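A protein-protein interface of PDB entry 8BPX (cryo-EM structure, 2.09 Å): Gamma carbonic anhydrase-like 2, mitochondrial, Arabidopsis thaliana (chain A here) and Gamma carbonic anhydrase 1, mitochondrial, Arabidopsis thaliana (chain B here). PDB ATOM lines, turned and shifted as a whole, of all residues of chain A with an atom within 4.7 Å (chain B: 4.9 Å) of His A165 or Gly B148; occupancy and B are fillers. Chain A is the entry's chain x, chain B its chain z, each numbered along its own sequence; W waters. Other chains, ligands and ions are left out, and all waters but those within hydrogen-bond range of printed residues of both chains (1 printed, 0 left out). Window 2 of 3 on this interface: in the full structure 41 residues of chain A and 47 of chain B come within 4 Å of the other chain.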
ATOM      1  N   ALA A 147      -2.021  29.313   5.700  1.00  0.00           N
ATOM      2  CA  ALA A 147      -1.472  29.249   7.076  1.00  0.00           C
ATOM      3  C   ALA A 147      -1.777  27.926   7.815  1.00  0.00           C
ATOM      4  O   ALA A 147      -2.793  27.293   7.541  1.00  0.00           O
ATOM      5  CB  ALA A 147      -1.940  30.431   7.886  1.00  0.00           C
ATOM      6  N   TYR A 148      -0.840  27.491   8.628  1.00  0.00           N
ATOM      7  CA  TYR A 148      -1.034  26.320   9.516  1.00  0.00           C
ATOM      8  C   TYR A 148      -1.121  25.023   8.722  1.00  0.00           C
ATOM      9  O   TYR A 148      -1.710  24.150   9.217  1.00  0.00           O
ATOM     10  CB  TYR A 148      -2.220  26.573  10.478  1.00  0.00           C
ATOM     11  CG  TYR A 148      -1.818  26.468  11.919  1.00  0.00           C
ATOM     12  CD1 TYR A 148      -1.371  25.260  12.433  1.00  0.00           C
ATOM     13  CD2 TYR A 148      -1.826  27.574  12.749  1.00  0.00           C
ATOM     14  CE1 TYR A 148      -0.965  25.151  13.750  1.00  0.00           C
ATOM     15  CE2 TYR A 148      -1.426  27.481  14.069  1.00  0.00           C
ATOM     16  CZ  TYR A 148      -0.990  26.263  14.565  1.00  0.00           C
ATOM     17  OH  TYR A 148      -0.585  26.132  15.849  1.00  0.00           O
ATOM     18  N   SER A 149      -0.582  25.030   7.524  1.00  0.00           N
ATOM     19  CA  SER A 149      -0.553  23.820   6.689  1.00  0.00           C
ATOM     20  C   SER A 149       0.711  22.961   6.904  1.00  0.00           C
ATOM     21  O   SER A 149       1.723  23.493   7.201  1.00  0.00           O
ATOM     22  CB  SER A 149      -0.906  24.143   5.229  1.00  0.00           C
ATOM     23  OG  SER A 149      -2.230  24.585   5.091  1.00  0.00           O
ATOM     24  N   GLY A 163      -5.763  25.360   1.096  1.00  0.00           N
ATOM     25  CA  GLY A 163      -6.516  26.012   2.146  1.00  0.00           C
ATOM     26  C   GLY A 163      -5.806  25.959   3.486  1.00  0.00           C
ATOM     27  O   GLY A 163      -4.923  25.135   3.727  1.00  0.00           O
ATOM     28  N   GLN A 164      -6.207  26.868   4.373  1.00  0.00           N
ATOM     29  CA  GLN A 164      -5.626  26.937   5.708  1.00  0.00           C
ATOM     30  C   GLN A 164      -5.799  25.614   6.448  1.00  0.00           C
ATOM     31  O   GLN A 164      -6.784  24.899   6.265  1.00  0.00           O
ATOM     32  CB  GLN A 164      -6.282  28.055   6.522  1.00  0.00           C
ATOM     33  CG  GLN A 164      -5.821  29.452   6.174  1.00  0.00           C
ATOM     34  CD  GLN A 164      -6.592  30.510   6.934  1.00  0.00           C
ATOM     35  OE1 GLN A 164      -6.262  30.832   8.071  1.00  0.00           O
ATOM     36  NE2 GLN A 164      -7.627  31.055   6.308  1.00  0.00           N
ATOM     37  N   HIS A 165      -4.836  25.263   7.301  1.00  0.00           N
ATOM     38  CA  HIS A 165      -4.924  24.122   8.249  1.00  0.00           C
ATOM     39  C   HIS A 165      -5.070  22.801   7.489  1.00  0.00           C
ATOM     40  O   HIS A 165      -5.747  21.950   7.951  1.00  0.00           O
ATOM     41  CB  HIS A 165      -6.024  24.401   9.305  1.00  0.00           C
ATOM     42  CG  HIS A 165      -5.705  23.831  10.631  1.00  0.00           C
ATOM     43  ND1 HIS A 165      -6.139  22.584  11.021  1.00  0.00           N
ATOM     44  CD2 HIS A 165      -4.933  24.299  11.627  1.00  0.00           C
ATOM     45  CE1 HIS A 165      -5.675  22.328  12.228  1.00  0.00           C
ATOM     46  NE2 HIS A 165      -4.936  23.365  12.613  1.00  0.00           N
ATOM     47  N   SER A 166      -4.461  22.705   6.337  1.00  0.00           N
ATOM     48  CA  SER A 166      -4.432  21.484   5.523  1.00  0.00           C
ATOM     49  C   SER A 166      -3.206  20.602   5.764  1.00  0.00           C
ATOM     50  O   SER A 166      -2.123  21.099   6.132  1.00  0.00           O
ATOM     51  CB  SER A 166      -4.611  21.874   4.034  1.00  0.00           C
ATOM     52  OG  SER A 166      -5.934  22.296   3.769  1.00  0.00           O
ATOM     53  N   ILE A 167      -3.305  19.366   5.372  1.00  0.00           N
ATOM     54  CA  ILE A 167      -2.231  18.400   5.569  1.00  0.00           C
ATOM     55  C   ILE A 167      -2.021  17.622   4.275  1.00  0.00           C
ATOM     56  O   ILE A 167      -2.966  17.027   3.743  1.00  0.00           O
ATOM     57  CB  ILE A 167      -2.523  17.449   6.741  1.00  0.00           C
ATOM     58  CG1 ILE A 167      -2.693  18.251   8.033  1.00  0.00           C
ATOM     59  CG2 ILE A 167      -1.413  16.420   6.882  1.00  0.00           C
ATOM     60  CD1 ILE A 167      -3.073  17.426   9.234  1.00  0.00           C
ATOM     61  N   GLY A 183      -8.755  22.880   5.975  1.00  0.00           N
ATOM     62  CA  GLY A 183      -8.948  21.693   6.779  1.00  0.00           C
ATOM     63  C   GLY A 183      -8.870  20.380   6.034  1.00  0.00           C
ATOM     64  O   GLY A 183      -9.263  19.350   6.591  1.00  0.00           O
ATOM     65  N   SER A 184      -8.382  20.376   4.799  1.00  0.00           N
ATOM     66  CA  SER A 184      -8.302  19.149   4.025  1.00  0.00           C
ATOM     67  C   SER A 184      -7.133  18.287   4.487  1.00  0.00           C
ATOM     68  O   SER A 184      -6.094  18.789   4.925  1.00  0.00           O
ATOM     69  CB  SER A 184      -8.159  19.461   2.537  1.00  0.00           C
ATOM     70  OG  SER A 184      -9.233  20.254   2.071  1.00  0.00           O
ATOM     71  N   GLY B 129      -8.393  28.365  22.267  1.00  0.00           N
ATOM     72  CA  GLY B 129      -7.584  27.211  22.597  1.00  0.00           C
ATOM     73  C   GLY B 129      -6.294  27.137  21.803  1.00  0.00           C
ATOM     74  O   GLY B 129      -6.089  27.830  20.807  1.00  0.00           O
ATOM     75  N   HIS B 130      -5.391  26.351  22.370  1.00  0.00           N
ATOM     76  CA  HIS B 130      -4.111  26.032  21.685  1.00  0.00           C
ATOM     77  C   HIS B 130      -4.227  25.765  20.189  1.00  0.00           C
ATOM     78  O   HIS B 130      -5.118  25.028  19.800  1.00  0.00           O
ATOM     79  CB  HIS B 130      -3.451  24.804  22.372  1.00  0.00           C
ATOM     80  CG  HIS B 130      -3.098  25.022  23.783  1.00  0.00           C
ATOM     81  ND1 HIS B 130      -2.180  25.955  24.150  1.00  0.00           N
ATOM     82  CD2 HIS B 130      -3.513  24.416  24.900  1.00  0.00           C
ATOM     83  CE1 HIS B 130      -2.030  25.915  25.439  1.00  0.00           C
ATOM     84  NE2 HIS B 130      -2.803  24.984  25.903  1.00  0.00           N
ATOM     85  N   SER B 131      -3.430  26.443  19.379  1.00  0.00           N
ATOM     86  CA  SER B 131      -3.301  26.132  17.939  1.00  0.00           C
ATOM     87  C   SER B 131      -4.611  26.323  17.168  1.00  0.00           C
ATOM     88  O   SER B 131      -4.783  25.695  16.209  1.00  0.00           O
ATOM     89  CB  SER B 131      -2.669  24.730  17.741  1.00  0.00           C
ATOM     90  OG  SER B 131      -1.566  24.516  18.611  1.00  0.00           O
ATOM     91  N   ALA B 132      -5.428  27.197  17.667  1.00  0.00           N
ATOM     92  CA  ALA B 132      -6.621  27.580  16.932  1.00  0.00           C
ATOM     93  C   ALA B 132      -6.267  28.590  15.846  1.00  0.00           C
ATOM     94  O   ALA B 132      -5.272  29.313  15.933  1.00  0.00           O
ATOM     95  CB  ALA B 132      -7.673  28.163  17.876  1.00  0.00           C
ATOM     96  N   VAL B 133      -7.096  28.590  14.800  1.00  0.00           N
ATOM     97  CA  VAL B 133      -6.959  29.548  13.697  1.00  0.00           C
ATOM     98  C   VAL B 133      -8.185  30.457  13.595  1.00  0.00           C
ATOM     99  O   VAL B 133      -9.262  29.978  13.376  1.00  0.00           O
ATOM    100  CB  VAL B 133      -6.616  28.881  12.353  1.00  0.00           C
ATOM    101  CG1 VAL B 133      -6.492  29.917  11.251  1.00  0.00           C
ATOM    102  CG2 VAL B 133      -5.326  28.073  12.448  1.00  0.00           C
ATOM    103  N   GLY B 146     -12.609  26.048  20.940  1.00  0.00           N
ATOM    104  CA  GLY B 146     -11.829  24.871  21.261  1.00  0.00           C
ATOM    105  C   GLY B 146     -10.497  24.872  20.540  1.00  0.00           C
ATOM    106  O   GLY B 146     -10.331  25.473  19.481  1.00  0.00           O
ATOM    107  N   MET B 147      -9.525  24.197  21.135  1.00  0.00           N
ATOM    108  CA  MET B 147      -8.181  24.260  20.590  1.00  0.00           C
ATOM    109  C   MET B 147      -8.107  23.481  19.279  1.00  0.00           C
ATOM    110  O   MET B 147      -8.839  22.511  19.071  1.00  0.00           O
ATOM    111  CB  MET B 147      -7.169  23.762  21.627  1.00  0.00           C
ATOM    112  CG  MET B 147      -7.223  22.297  22.003  1.00  0.00           C
ATOM    113  SD  MET B 147      -5.869  21.869  23.084  1.00  0.00           S
ATOM    114  CE  MET B 147      -4.580  21.767  21.841  1.00  0.00           C
ATOM    115  N   GLY B 148      -7.239  23.933  18.379  1.00  0.00           N
ATOM    116  CA  GLY B 148      -7.151  23.331  17.067  1.00  0.00           C
ATOM    117  C   GLY B 148      -8.320  23.614  16.151  1.00  0.00           C
ATOM    118  O   GLY B 148      -8.370  23.062  15.050  1.00  0.00           O
ATOM    119  N   ALA B 149      -9.265  24.451  16.569  1.00  0.00           N
ATOM    120  CA  ALA B 149     -10.393  24.807  15.725  1.00  0.00           C
ATOM    121  C   ALA B 149     -10.005  25.902  14.734  1.00  0.00           C
ATOM    122  O   ALA B 149      -9.066  26.671  14.952  1.00  0.00           O
ATOM    123  CB  ALA B 149     -11.577  25.266  16.573  1.00  0.00           C
ATOM    124  N   THR B 150     -10.754  25.969  13.635  1.00  0.00           N
ATOM    125  CA  THR B 150     -10.521  26.950  12.584  1.00  0.00           C
ATOM    126  C   THR B 150     -11.811  27.706  12.301  1.00  0.00           C
ATOM    127  O   THR B 150     -12.847  27.093  12.027  1.00  0.00           O
ATOM    128  CB  THR B 150     -10.008  26.280  11.303  1.00  0.00           C
ATOM    129  OG1 THR B 150      -8.819  25.534  11.591  1.00  0.00           O
ATOM    130  CG2 THR B 150      -9.702  27.317  10.234  1.00  0.00           C
ATOM    131  N   GLY B 166     -10.940  21.220  17.326  1.00  0.00           N
ATOM    132  CA  GLY B 166     -10.772  20.672  15.997  1.00  0.00           C
ATOM    133  C   GLY B 166     -11.888  20.962  15.020  1.00  0.00           C
ATOM    134  O   GLY B 166     -11.907  20.369  13.940  1.00  0.00           O
ATOM    135  N   ALA B 167     -12.818  21.851  15.358  1.00  0.00           N
ATOM    136  CA  ALA B 167     -13.928  22.168  14.470  1.00  0.00           C
ATOM    137  C   ALA B 167     -13.473  23.076  13.328  1.00  0.00           C
ATOM    138  O   ALA B 167     -12.474  23.791  13.426  1.00  0.00           O
ATOM    139  CB  ALA B 167     -15.065  22.833  15.242  1.00  0.00           C
HETATM  140  O   HOH W   1      -3.768  23.309  15.047  1.00  0.00           O
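The side-chain hydroxyl of Tyr A148 lies close to the side-chain hydroxyl of Ser B131, at 3.3 Å.
Of the 12 printed residues of chain B, 4 touch a printed residue of chain A. Among the printed residues, 6 pairs touch across the chains.
Val B133 touches Tyr A148. Gln A164 touches Val B133 (OE1 to CG1, 3.3 Å). CD2 of His A165 touches CG2 of Val B133, 3.9 Å away. His A165 touches Gly B148. CG of His A165 touches OG1 of Thr B150, at 3.7 Å.
Water W1 bridges a ring nitrogen (NE2) of His A165 and the backbone carbonyl oxygen (O) of Ser B131.
The backbone carbonyl oxygen of Ala A147 sits at hydrogen-bond distance from the backbone NH of His A165. The side-chain hydroxyl (OG) of Ser A149 lies within hydrogen-bond range of the backbone NH (N) of His A165. N of Gly A183 lies within hydrogen-bond range of O of Gln A164 (2.8 Å). N of Gly B148 sits at hydrogen-bond distance from O of His B130, at 2.8 Å. The backbone NH of Val B133 lies within hydrogen-bond range of the backbone carbonyl oxygen of Ala B149 (2.8 Å). N of Thr B150 sits at hydrogen-bond distance from O of Ala B167, at 2.8 Å.
His A165 touches just these residues of chain B: Val B133, Gly B148 and Thr B150. Gly B148 touches one residue of chain A. Of the printed residues of chain A, Val B133 touches Tyr A148 (3.5 Å), Gln A164 (3.3 Å) and His A165 (3.9 Å). Of the printed residues of chain A, Ser B131 touches Tyr A148 (3.1 Å). Gly B166 touches none of the printed residues of chain A. Ala B149 touches none of the printed residues of chain A. The nearest residue of chain B that does not touch His A165 is Ser B131 (4.3 Å).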
